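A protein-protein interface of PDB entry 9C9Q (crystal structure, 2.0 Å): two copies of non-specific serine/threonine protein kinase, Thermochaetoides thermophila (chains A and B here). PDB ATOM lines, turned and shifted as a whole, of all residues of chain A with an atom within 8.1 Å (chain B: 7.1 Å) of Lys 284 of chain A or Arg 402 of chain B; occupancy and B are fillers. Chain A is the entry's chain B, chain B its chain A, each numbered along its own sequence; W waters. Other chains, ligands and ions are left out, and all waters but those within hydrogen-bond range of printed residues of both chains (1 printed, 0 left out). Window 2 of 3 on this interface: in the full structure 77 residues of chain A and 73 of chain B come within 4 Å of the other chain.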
ATOM      1  N   MET A 148       1.547  29.518 -14.681  1.00  0.00           N
ATOM      2  CA  MET A 148       2.778  28.770 -14.451  1.00  0.00           C
ATOM      3  C   MET A 148       3.554  29.356 -13.277  1.00  0.00           C
ATOM      4  O   MET A 148       3.644  30.579 -13.122  1.00  0.00           O
ATOM      5  CB  MET A 148       3.666  28.773 -15.702  1.00  0.00           C
ATOM      6  CG  MET A 148       3.021  28.168 -16.947  1.00  0.00           C
ATOM      7  SD  MET A 148       4.214  27.691 -18.234  1.00  0.00           S
ATOM      8  CE  MET A 148       4.751  29.281 -18.869  1.00  0.00           C
ATOM      9  N   ASP A 149       4.112  28.469 -12.449  1.00  0.00           N
ATOM     10  CA  ASP A 149       5.051  28.858 -11.394  1.00  0.00           C
ATOM     11  C   ASP A 149       4.421  29.845 -10.426  1.00  0.00           C
ATOM     12  O   ASP A 149       5.061  30.802  -9.969  1.00  0.00           O
ATOM     13  CB  ASP A 149       6.354  29.405 -11.984  1.00  0.00           C
ATOM     14  CG  ASP A 149       7.118  28.332 -12.726  1.00  0.00           C
ATOM     15  OD1 ASP A 149       7.392  27.263 -12.111  1.00  0.00           O
ATOM     16  OD2 ASP A 149       7.379  28.530 -13.931  1.00  0.00           O
ATOM     17  N   LEU A 150       3.158  29.577 -10.088  1.00  0.00           N
ATOM     18  CA  LEU A 150       2.423  30.477  -9.221  1.00  0.00           C
ATOM     19  C   LEU A 150       3.095  30.601  -7.867  1.00  0.00           C
ATOM     20  O   LEU A 150       3.221  31.715  -7.336  1.00  0.00           O
ATOM     21  CB  LEU A 150       0.971  30.012  -9.092  1.00  0.00           C
ATOM     22  CG  LEU A 150       0.173  30.378 -10.343  1.00  0.00           C
ATOM     23  CD1 LEU A 150      -1.315  30.408 -10.071  1.00  0.00           C
ATOM     24  CD2 LEU A 150       0.635  31.708 -10.925  1.00  0.00           C
ATOM     25  N   MET A 152       6.253  30.250  -7.247  1.00  0.00           N
ATOM     26  CA  MET A 152       7.527  30.950  -7.367  1.00  0.00           C
ATOM     27  C   MET A 152       7.329  32.471  -7.389  1.00  0.00           C
ATOM     28  O   MET A 152       8.095  33.199  -6.751  1.00  0.00           O
ATOM     29  CB  MET A 152       8.260  30.473  -8.618  1.00  0.00           C
ATOM     30  CG  MET A 152       9.731  30.901  -8.658  1.00  0.00           C
ATOM     31  SD  MET A 152      10.427  30.613 -10.296  1.00  0.00           S
ATOM     32  CE  MET A 152       9.568  31.871 -11.235  1.00  0.00           C
ATOM     33  N   ALA A 155       6.807  33.612  -3.918  1.00  0.00           N
ATOM     34  CA  ALA A 155       8.062  33.705  -3.164  1.00  0.00           C
ATOM     35  C   ALA A 155       8.892  34.923  -3.563  1.00  0.00           C
ATOM     36  O   ALA A 155       9.601  35.497  -2.722  1.00  0.00           O
ATOM     37  CB  ALA A 155       8.879  32.423  -3.366  1.00  0.00           C
ATOM     38  N   LYS A 159      10.315  37.775  -1.165  1.00  0.00           N
ATOM     39  CA  LYS A 159      11.709  38.179  -1.279  1.00  0.00           C
ATOM     40  C   LYS A 159      11.850  39.694  -1.327  1.00  0.00           C
ATOM     41  O   LYS A 159      12.728  40.258  -0.665  1.00  0.00           O
ATOM     42  CB  LYS A 159      12.333  37.528  -2.521  1.00  0.00           C
ATOM     43  CG  LYS A 159      13.753  37.997  -2.853  1.00  0.00           C
ATOM     44  CD  LYS A 159      14.806  37.528  -1.842  1.00  0.00           C
ATOM     45  CE  LYS A 159      16.206  38.052  -2.197  1.00  0.00           C
ATOM     46  NZ  LYS A 159      17.187  37.869  -1.094  1.00  0.00           N
ATOM     47  N   GLU A 277       6.053  24.505  -1.425  1.00  0.00           N
ATOM     48  CA  GLU A 277       6.769  25.016  -2.590  1.00  0.00           C
ATOM     49  C   GLU A 277       7.178  26.477  -2.407  1.00  0.00           C
ATOM     50  O   GLU A 277       8.318  26.857  -2.706  1.00  0.00           O
ATOM     51  CB  GLU A 277       5.875  24.846  -3.816  1.00  0.00           C
ATOM     52  CG  GLU A 277       6.577  24.761  -5.138  1.00  0.00           C
ATOM     53  CD  GLU A 277       5.659  24.214  -6.212  1.00  0.00           C
ATOM     54  OE1 GLU A 277       4.574  23.704  -5.849  1.00  0.00           O
ATOM     55  OE2 GLU A 277       6.019  24.294  -7.410  1.00  0.00           O
ATOM     56  N   VAL A 278       6.265  27.310  -1.907  1.00  0.00           N
ATOM     57  CA  VAL A 278       6.611  28.695  -1.604  1.00  0.00           C
ATOM     58  C   VAL A 278       7.763  28.740  -0.615  1.00  0.00           C
ATOM     59  O   VAL A 278       8.742  29.480  -0.796  1.00  0.00           O
ATOM     60  CB  VAL A 278       5.383  29.450  -1.067  1.00  0.00           C
ATOM     61  CG1 VAL A 278       5.764  30.905  -0.694  1.00  0.00           C
ATOM     62  CG2 VAL A 278       4.269  29.416  -2.089  1.00  0.00           C
ATOM     63  N   TYR A 279       7.662  27.949   0.452  1.00  0.00           N
ATOM     64  CA  TYR A 279       8.714  27.929   1.460  1.00  0.00           C
ATOM     65  C   TYR A 279      10.055  27.524   0.857  1.00  0.00           C
ATOM     66  O   TYR A 279      11.100  28.088   1.207  1.00  0.00           O
ATOM     67  CB  TYR A 279       8.336  26.971   2.584  1.00  0.00           C
ATOM     68  CG  TYR A 279       9.421  26.821   3.620  1.00  0.00           C
ATOM     69  CD1 TYR A 279       9.907  27.933   4.308  1.00  0.00           C
ATOM     70  CD2 TYR A 279       9.951  25.571   3.923  1.00  0.00           C
ATOM     71  CE1 TYR A 279      10.888  27.809   5.266  1.00  0.00           C
ATOM     72  CE2 TYR A 279      10.938  25.426   4.882  1.00  0.00           C
ATOM     73  CZ  TYR A 279      11.399  26.543   5.551  1.00  0.00           C
ATOM     74  OH  TYR A 279      12.376  26.403   6.498  1.00  0.00           O
ATOM     75  N   GLU A 280      10.044  26.550  -0.052  1.00  0.00           N
ATOM     76  CA  GLU A 280      11.298  26.103  -0.641  1.00  0.00           C
ATOM     77  C   GLU A 280      11.882  27.172  -1.555  1.00  0.00           C
ATOM     78  O   GLU A 280      13.101  27.374  -1.574  1.00  0.00           O
ATOM     79  CB  GLU A 280      11.093  24.794  -1.405  1.00  0.00           C
ATOM     80  CG  GLU A 280      10.831  23.582  -0.508  1.00  0.00           C
ATOM     81  CD  GLU A 280      11.984  23.285   0.448  1.00  0.00           C
ATOM     82  OE1 GLU A 280      13.162  23.536   0.078  1.00  0.00           O
ATOM     83  OE2 GLU A 280      11.714  22.806   1.575  1.00  0.00           O
ATOM     84  N   TYR A 281      11.031  27.846  -2.339  1.00  0.00           N
ATOM     85  CA  TYR A 281      11.524  28.932  -3.184  1.00  0.00           C
ATOM     86  C   TYR A 281      12.103  30.056  -2.345  1.00  0.00           C
ATOM     87  O   TYR A 281      13.155  30.615  -2.685  1.00  0.00           O
ATOM     88  CB  TYR A 281      10.414  29.451  -4.088  1.00  0.00           C
ATOM     89  CG  TYR A 281      10.275  28.608  -5.312  1.00  0.00           C
ATOM     90  CD1 TYR A 281      11.387  28.310  -6.087  1.00  0.00           C
ATOM     91  CD2 TYR A 281       9.054  28.063  -5.671  1.00  0.00           C
ATOM     92  CE1 TYR A 281      11.284  27.523  -7.198  1.00  0.00           C
ATOM     93  CE2 TYR A 281       8.946  27.267  -6.789  1.00  0.00           C
ATOM     94  CZ  TYR A 281      10.064  27.000  -7.539  1.00  0.00           C
ATOM     95  OH  TYR A 281       9.962  26.216  -8.654  1.00  0.00           O
ATOM     96  N   SER A 282      11.448  30.382  -1.229  1.00  0.00           N
ATOM     97  CA  SER A 282      11.973  31.421  -0.342  1.00  0.00           C
ATOM     98  C   SER A 282      13.375  31.084   0.147  1.00  0.00           C
ATOM     99  O   SER A 282      14.200  31.984   0.344  1.00  0.00           O
ATOM    100  CB  SER A 282      11.040  31.620   0.848  1.00  0.00           C
ATOM    101  OG  SER A 282       9.734  31.907   0.385  1.00  0.00           O
ATOM    102  N   LYS A 283      13.657  29.792   0.367  1.00  0.00           N
ATOM    103  CA  LYS A 283      15.016  29.393   0.723  1.00  0.00           C
ATOM    104  C   LYS A 283      15.973  29.609  -0.440  1.00  0.00           C
ATOM    105  O   LYS A 283      17.088  30.103  -0.246  1.00  0.00           O
ATOM    106  CB  LYS A 283      15.042  27.933   1.200  1.00  0.00           C
ATOM    107  CG  LYS A 283      14.518  27.774   2.625  1.00  0.00           C
ATOM    108  CD  LYS A 283      14.870  26.424   3.255  1.00  0.00           C
ATOM    109  CE  LYS A 283      13.952  25.326   2.766  1.00  0.00           C
ATOM    110  NZ  LYS A 283      14.211  24.026   3.456  1.00  0.00           N
ATOM    111  N   LYS A 284      15.548  29.279  -1.663  1.00  0.00           N
ATOM    112  CA  LYS A 284      16.398  29.528  -2.825  1.00  0.00           C
ATOM    113  C   LYS A 284      16.665  31.026  -3.029  1.00  0.00           C
ATOM    114  O   LYS A 284      17.782  31.420  -3.391  1.00  0.00           O
ATOM    115  CB  LYS A 284      15.761  28.898  -4.064  1.00  0.00           C
ATOM    116  CG  LYS A 284      15.710  27.339  -4.014  1.00  0.00           C
ATOM    117  CD  LYS A 284      15.121  26.744  -5.286  1.00  0.00           C
ATOM    118  CE  LYS A 284      14.748  25.267  -5.100  1.00  0.00           C
ATOM    119  NZ  LYS A 284      14.165  24.632  -6.326  1.00  0.00           N
ATOM    120  N   PHE A 285      15.653  31.879  -2.813  1.00  0.00           N
ATOM    121  CA  PHE A 285      15.823  33.332  -2.895  1.00  0.00           C
ATOM    122  C   PHE A 285      16.629  33.913  -1.739  1.00  0.00           C
ATOM    123  O   PHE A 285      16.907  35.122  -1.744  1.00  0.00           O
ATOM    124  CB  PHE A 285      14.452  34.011  -2.930  1.00  0.00           C
ATOM    125  CG  PHE A 285      13.785  33.978  -4.279  1.00  0.00           C
ATOM    126  CD1 PHE A 285      14.446  34.434  -5.409  1.00  0.00           C
ATOM    127  CD2 PHE A 285      12.497  33.482  -4.411  1.00  0.00           C
ATOM    128  CE1 PHE A 285      13.820  34.410  -6.660  1.00  0.00           C
ATOM    129  CE2 PHE A 285      11.866  33.444  -5.648  1.00  0.00           C
ATOM    130  CZ  PHE A 285      12.520  33.915  -6.774  1.00  0.00           C
ATOM    131  N   LYS A 286      16.983  33.097  -0.740  1.00  0.00           N
ATOM    132  CA  LYS A 286      17.741  33.525   0.436  1.00  0.00           C
ATOM    133  C   LYS A 286      16.981  34.586   1.229  1.00  0.00           C
ATOM    134  O   LYS A 286      17.478  35.685   1.469  1.00  0.00           O
ATOM    135  CB  LYS A 286      19.133  34.048   0.053  1.00  0.00           C
ATOM    136  CG  LYS A 286      20.039  33.033  -0.606  1.00  0.00           C
ATOM    137  CD  LYS A 286      20.438  31.952   0.371  1.00  0.00           C
ATOM    138  CE  LYS A 286      21.787  31.337  -0.003  1.00  0.00           C
ATOM    139  NZ  LYS A 286      21.646  30.014  -0.680  1.00  0.00           N
ATOM    140  N   VAL A 287      15.760  34.245   1.627  1.00  0.00           N
ATOM    141  CA  VAL A 287      15.001  35.088   2.543  1.00  0.00           C
ATOM    142  C   VAL A 287      15.577  34.898   3.939  1.00  0.00           C
ATOM    143  O   VAL A 287      15.620  33.777   4.456  1.00  0.00           O
ATOM    144  CB  VAL A 287      13.504  34.741   2.506  1.00  0.00           C
ATOM    145  CG1 VAL A 287      12.750  35.492   3.591  1.00  0.00           C
ATOM    146  CG2 VAL A 287      12.915  35.036   1.132  1.00  0.00           C
ATOM    147  N   SER B 395      17.589  28.733 -18.714  1.00  0.00           N
ATOM    148  CA  SER B 395      18.148  27.390 -18.753  1.00  0.00           C
ATOM    149  C   SER B 395      17.198  26.532 -19.561  1.00  0.00           C
ATOM    150  O   SER B 395      15.989  26.777 -19.578  1.00  0.00           O
ATOM    151  CB  SER B 395      18.344  26.807 -17.347  1.00  0.00           C
ATOM    152  OG  SER B 395      18.911  25.493 -17.411  1.00  0.00           O
ATOM    153  N   ASP B 397      17.029  23.312 -18.926  1.00  0.00           N
ATOM    154  CA  ASP B 397      16.638  22.255 -17.999  1.00  0.00           C
ATOM    155  C   ASP B 397      15.748  22.877 -16.930  1.00  0.00           C
ATOM    156  O   ASP B 397      16.237  23.685 -16.125  1.00  0.00           O
ATOM    157  CB  ASP B 397      17.881  21.620 -17.375  1.00  0.00           C
ATOM    158  CG  ASP B 397      17.562  20.414 -16.508  1.00  0.00           C
ATOM    159  OD1 ASP B 397      16.454  20.348 -15.935  1.00  0.00           O
ATOM    160  OD2 ASP B 397      18.440  19.529 -16.390  1.00  0.00           O
ATOM    161  N   PRO B 398      14.457  22.531 -16.872  1.00  0.00           N
ATOM    162  CA  PRO B 398      13.550  23.218 -15.932  1.00  0.00           C
ATOM    163  C   PRO B 398      13.958  23.095 -14.477  1.00  0.00           C
ATOM    164  O   PRO B 398      13.654  24.003 -13.694  1.00  0.00           O
ATOM    165  CB  PRO B 398      12.197  22.538 -16.191  1.00  0.00           C
ATOM    166  CG  PRO B 398      12.291  22.030 -17.610  1.00  0.00           C
ATOM    167  CD  PRO B 398      13.738  21.630 -17.790  1.00  0.00           C
ATOM    168  N   SER B 399      14.620  22.002 -14.072  1.00  0.00           N
ATOM    169  CA  SER B 399      15.007  21.886 -12.670  1.00  0.00           C
ATOM    170  C   SER B 399      16.251  22.711 -12.348  1.00  0.00           C
ATOM    171  O   SER B 399      16.408  23.184 -11.212  1.00  0.00           O
ATOM    172  CB  SER B 399      15.250  20.423 -12.308  1.00  0.00           C
ATOM    173  OG  SER B 399      16.380  19.952 -13.011  1.00  0.00           O
ATOM    174  N   ILE B 400      17.148  22.879 -13.314  1.00  0.00           N
ATOM    175  CA  ILE B 400      18.260  23.814 -13.147  1.00  0.00           C
ATOM    176  C   ILE B 400      17.742  25.254 -13.111  1.00  0.00           C
ATOM    177  O   ILE B 400      18.161  26.061 -12.274  1.00  0.00           O
ATOM    178  CB  ILE B 400      19.285  23.619 -14.275  1.00  0.00           C
ATOM    179  CG1 ILE B 400      20.082  22.329 -14.057  1.00  0.00           C
ATOM    180  CG2 ILE B 400      20.213  24.826 -14.365  1.00  0.00           C
ATOM    181  CD1 ILE B 400      21.070  22.076 -15.152  1.00  0.00           C
ATOM    182  N   LEU B 401      16.827  25.592 -14.022  1.00  0.00           N
ATOM    183  CA  LEU B 401      16.221  26.930 -14.015  1.00  0.00           C
ATOM    184  C   LEU B 401      15.658  27.271 -12.644  1.00  0.00           C
ATOM    185  O   LEU B 401      15.821  28.392 -12.157  1.00  0.00           O
ATOM    186  CB  LEU B 401      15.114  27.016 -15.060  1.00  0.00           C
ATOM    187  CG  LEU B 401      14.353  28.348 -15.190  1.00  0.00           C
ATOM    188  CD1 LEU B 401      15.279  29.377 -15.748  1.00  0.00           C
ATOM    189  CD2 LEU B 401      13.147  28.178 -16.089  1.00  0.00           C
ATOM    190  N   ARG B 402      15.010  26.304 -11.990  1.00  0.00           N
ATOM    191  CA  ARG B 402      14.301  26.577 -10.747  1.00  0.00           C
ATOM    192  C   ARG B 402      15.130  26.267  -9.516  1.00  0.00           C
ATOM    193  O   ARG B 402      14.616  26.377  -8.397  1.00  0.00           O
ATOM    194  CB  ARG B 402      12.979  25.804 -10.715  1.00  0.00           C
ATOM    195  CG  ARG B 402      11.961  26.346 -11.719  1.00  0.00           C
ATOM    196  CD  ARG B 402      10.754  25.440 -11.851  1.00  0.00           C
ATOM    197  NE  ARG B 402       9.797  25.965 -12.817  1.00  0.00           N
ATOM    198  CZ  ARG B 402       9.929  25.893 -14.134  1.00  0.00           C
ATOM    199  NH1 ARG B 402      10.978  25.307 -14.694  1.00  0.00           N
ATOM    200  NH2 ARG B 402       8.985  26.424 -14.913  1.00  0.00           N
ATOM    201  N   SER B 403      16.398  25.892  -9.701  1.00  0.00           N
ATOM    202  CA  SER B 403      17.336  25.724  -8.594  1.00  0.00           C
ATOM    203  C   SER B 403      18.517  26.677  -8.754  1.00  0.00           C
ATOM    204  O   SER B 403      18.608  27.658  -8.012  1.00  0.00           O
ATOM    205  CB  SER B 403      17.803  24.269  -8.512  1.00  0.00           C
ATOM    206  OG  SER B 403      18.265  23.813  -9.779  1.00  0.00           O
ATOM    207  N   SER B 404      19.420  26.419  -9.703  1.00  0.00           N
ATOM    208  CA  SER B 404      20.553  27.316  -9.918  1.00  0.00           C
ATOM    209  C   SER B 404      20.094  28.691 -10.408  1.00  0.00           C
ATOM    210  O   SER B 404      20.678  29.713 -10.040  1.00  0.00           O
ATOM    211  CB  SER B 404      21.527  26.687 -10.913  1.00  0.00           C
ATOM    212  OG  SER B 404      22.196  25.590 -10.333  1.00  0.00           O
ATOM    213  N   GLY B 405      19.050  28.732 -11.239  1.00  0.00           N
ATOM    214  CA  GLY B 405      18.565  30.008 -11.747  1.00  0.00           C
ATOM    215  C   GLY B 405      18.159  30.971 -10.650  1.00  0.00           C
ATOM    216  O   GLY B 405      18.474  32.164 -10.704  1.00  0.00           O
ATOM    217  N   ILE B 406      17.427  30.476  -9.651  1.00  0.00           N
ATOM    218  CA  ILE B 406      17.001  31.335  -8.550  1.00  0.00           C
ATOM    219  C   ILE B 406      18.214  31.834  -7.775  1.00  0.00           C
ATOM    220  O   ILE B 406      18.264  32.992  -7.341  1.00  0.00           O
ATOM    221  CB  ILE B 406      16.019  30.585  -7.632  1.00  0.00           C
ATOM    222  CG1 ILE B 406      14.766  30.159  -8.412  1.00  0.00           C
ATOM    223  CG2 ILE B 406      15.649  31.453  -6.445  1.00  0.00           C
ATOM    224  CD1 ILE B 406      14.047  31.321  -9.051  1.00  0.00           C
ATOM    225  N   GLU B 407      19.210  30.965  -7.603  1.00  0.00           N
ATOM    226  CA  GLU B 407      20.402  31.310  -6.834  1.00  0.00           C
ATOM    227  C   GLU B 407      21.215  32.403  -7.510  1.00  0.00           C
ATOM    228  O   GLU B 407      21.719  33.307  -6.836  1.00  0.00           O
ATOM    229  CB  GLU B 407      21.270  30.066  -6.632  1.00  0.00           C
ATOM    230  CG  GLU B 407      21.632  29.825  -5.185  1.00  0.00           C
ATOM    231  CD  GLU B 407      20.396  29.663  -4.299  1.00  0.00           C
ATOM    232  OE1 GLU B 407      19.403  29.048  -4.756  1.00  0.00           O
ATOM    233  OE2 GLU B 407      20.414  30.166  -3.149  1.00  0.00           O
ATOM    234  N   LEU B 408      21.392  32.314  -8.827  1.00  0.00           N
ATOM    235  CA  LEU B 408      22.068  33.385  -9.549  1.00  0.00           C
ATOM    236  C   LEU B 408      21.264  34.672  -9.469  1.00  0.00           C
ATOM    237  O   LEU B 408      21.832  35.759  -9.310  1.00  0.00           O
ATOM    238  CB  LEU B 408      22.287  32.995 -11.008  1.00  0.00           C
ATOM    239  CG  LEU B 408      23.553  32.204 -11.323  1.00  0.00           C
ATOM    240  CD1 LEU B 408      23.521  31.691 -12.755  1.00  0.00           C
ATOM    241  CD2 LEU B 408      24.779  33.066 -11.086  1.00  0.00           C
ATOM    242  N   GLN B 410      19.101  35.846  -7.065  1.00  0.00           N
ATOM    243  CA  GLN B 410      19.259  36.547  -5.799  1.00  0.00           C
ATOM    244  C   GLN B 410      20.670  37.084  -5.644  1.00  0.00           C
ATOM    245  O   GLN B 410      20.874  38.116  -4.993  1.00  0.00           O
ATOM    246  CB  GLN B 410      18.900  35.626  -4.627  1.00  0.00           C
ATOM    247  CG  GLN B 410      19.891  34.489  -4.370  1.00  0.00           C
ATOM    248  CD  GLN B 410      20.953  34.849  -3.355  1.00  0.00           C
ATOM    249  OE1 GLN B 410      20.818  35.830  -2.618  1.00  0.00           O
ATOM    250  NE2 GLN B 410      22.018  34.049  -3.301  1.00  0.00           N
ATOM    251  N   MET B 411      21.653  36.417  -6.250  1.00  0.00           N
ATOM    252  CA  MET B 411      23.017  36.924  -6.161  1.00  0.00           C
ATOM    253  C   MET B 411      23.151  38.221  -6.946  1.00  0.00           C
ATOM    254  O   MET B 411      23.741  39.184  -6.451  1.00  0.00           O
ATOM    255  CB  MET B 411      24.014  35.869  -6.651  1.00  0.00           C
ATOM    256  CG  MET B 411      25.473  36.270  -6.457  1.00  0.00           C
ATOM    257  SD  MET B 411      26.073  37.299  -7.811  1.00  0.00           S
ATOM    258  CE  MET B 411      25.918  36.173  -9.199  1.00  0.00           C
ATOM    259  N   LEU B 421      13.957  36.039 -14.260  1.00  0.00           N
ATOM    260  CA  LEU B 421      14.039  34.630 -14.629  1.00  0.00           C
ATOM    261  C   LEU B 421      13.221  34.362 -15.884  1.00  0.00           C
ATOM    262  O   LEU B 421      12.084  34.822 -16.009  1.00  0.00           O
ATOM    263  CB  LEU B 421      13.532  33.741 -13.493  1.00  0.00           C
ATOM    264  CG  LEU B 421      13.879  32.257 -13.727  1.00  0.00           C
ATOM    265  CD1 LEU B 421      15.327  32.084 -13.339  1.00  0.00           C
ATOM    266  CD2 LEU B 421      12.958  31.301 -12.949  1.00  0.00           C
ATOM    267  N   ALA B 422      13.799  33.607 -16.815  1.00  0.00           N
ATOM    268  CA  ALA B 422      13.048  33.244 -18.001  1.00  0.00           C
ATOM    269  C   ALA B 422      12.057  32.136 -17.668  1.00  0.00           C
ATOM    270  O   ALA B 422      12.224  31.394 -16.693  1.00  0.00           O
ATOM    271  CB  ALA B 422      13.976  32.772 -19.122  1.00  0.00           C
ATOM    272  N   ARG B 423      11.022  32.021 -18.495  1.00  0.00           N
ATOM    273  CA  ARG B 423      10.198  30.826 -18.468  1.00  0.00           C
ATOM    274  C   ARG B 423      10.954  29.685 -19.146  1.00  0.00           C
ATOM    275  O   ARG B 423      12.054  29.862 -19.678  1.00  0.00           O
ATOM    276  CB  ARG B 423       8.857  31.078 -19.150  1.00  0.00           C
ATOM    277  CG  ARG B 423       8.993  31.437 -20.613  1.00  0.00           C
ATOM    278  CD  ARG B 423       7.819  32.283 -21.090  1.00  0.00           C
ATOM    279  NE  ARG B 423       6.589  31.507 -21.163  1.00  0.00           N
ATOM    280  CZ  ARG B 423       5.443  31.966 -21.649  1.00  0.00           C
ATOM    281  NH1 ARG B 423       5.336  33.199 -22.119  1.00  0.00           N
ATOM    282  NH2 ARG B 423       4.381  31.165 -21.667  1.00  0.00           N
ATOM    283  N   ASP B 424      10.354  28.498 -19.113  1.00  0.00           N
ATOM    284  CA  ASP B 424      10.981  27.322 -19.707  1.00  0.00           C
ATOM    285  C   ASP B 424      11.156  27.517 -21.207  1.00  0.00           C
ATOM    286  O   ASP B 424      10.307  28.110 -21.877  1.00  0.00           O
ATOM    287  CB  ASP B 424      10.138  26.065 -19.439  1.00  0.00           C
ATOM    288  CG  ASP B 424      10.290  25.536 -18.014  1.00  0.00           C
ATOM    289  OD1 ASP B 424      11.390  25.678 -17.426  1.00  0.00           O
ATOM    290  OD2 ASP B 424       9.310  24.956 -17.488  1.00  0.00           O
HETATM  291  O   HOH W   1      19.488  39.006  -2.657  1.00  0.00           O
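The side-chain amino group (NZ) of Lys 284 of chain A sits at hydrogen-bond distance from the backbone carbonyl oxygen (O) of Arg 402 of chain B, 2.7 Å away. The guanidinium group of Arg 402 of chain B lies within salt-bridge range of the side-chain carboxylate of Asp 149 of chain A, 2.8 Å away. O of Lys 284 of chain A sits close to OE2 of Glu 407 of chain B. The side-chain carboxylate (OE2) of Glu 407 of chain B lies within salt-bridge range of the side-chain amino group (NZ) of Lys 286 of chain A, at 2.8 Å.
NZ of Lys 159 of chain A is in hydrogen-bond range of O of Lys 286 of chain A (3.4 Å). NH1 of Arg 402 of chain B is in salt-bridge range of OD1 of Asp 424 of chain B (2.8 Å). The side-chain amino group (NZ) of Lys 159 of chain A is in hydrogen-bond range of the backbone carbonyl oxygen (O) of Phe 285 of chain A. The backbone carbonyl oxygen of Pro 398 of chain B lies within hydrogen-bond range of the guanidinium group of Arg 402 of chain B (3.1 Å).
Among the printed residues, pairs that only touch across the chains: Met 148 of chain A with Arg 423 of chain B (3.4 Å), Met 152 of chain A with Ile 406 of chain B (3.9 Å), Met 152 of chain A with Leu 421 of chain B (3.7 Å), Tyr 281 of chain A with Arg 402 of chain B (3.4 Å), Lys 284 of chain A with Ile 406 of chain B (3.5 Å), Lys 284 of chain A with Gln 410 of chain B (3.9 Å), Phe 285 of chain A with Ile 406 of chain B (3.4 Å), Phe 285 of chain A with Gln 410 of chain B (3.5 Å) and Lys 286 of chain A with Gln 410 of chain B (3.4 Å).
Of the printed residues of chain B, Lys 284 of chain A touches Arg 402, Ile 406, Glu 407 and Gln 410. Of chain A, only Asp 149 (2.8 Å), Tyr 281 (3.4 Å) and Lys 284 (2.7 Å) come within 4 Å of Arg 402 of chain B. Printed residues of chain A within 4 Å of Gln 410 of chain B: Lys 284, Phe 285 and Lys 286. Printed residues of chain B within 4 Å of Lys 286 of chain A: Glu 407 (2.8 Å) and Gln 410 (3.4 Å). Of the printed residues of chain A, Glu 407 of chain B touches Lys 284 and Lys 286. The nearest residue of chain A that does not touch Arg 402 of chain B is Met 152 of chain A (4.8 Å).
Of the 19 printed residues of chain B, 6 touch a printed residue of chain A. Among the printed residues, 13 pairs touch across the chains. Among the printed residues, Asp or Glu carboxylates within 4 Å of a Lys or Arg side-chain nitrogen of the other chain: Asp 149 of chain A with Arg 402 of chain B and Lys 286 of chain A with Glu 407 of chain B.
No position is printed for both chains. Of the 13 pairs that touch across the chains among the printed residues, none has its exchanged pair printed and touching as well.
Water W1 bridges O of Gln 410 of chain B (2.9 Å) and NZ of Lys 159 of chain A (3.0 Å).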
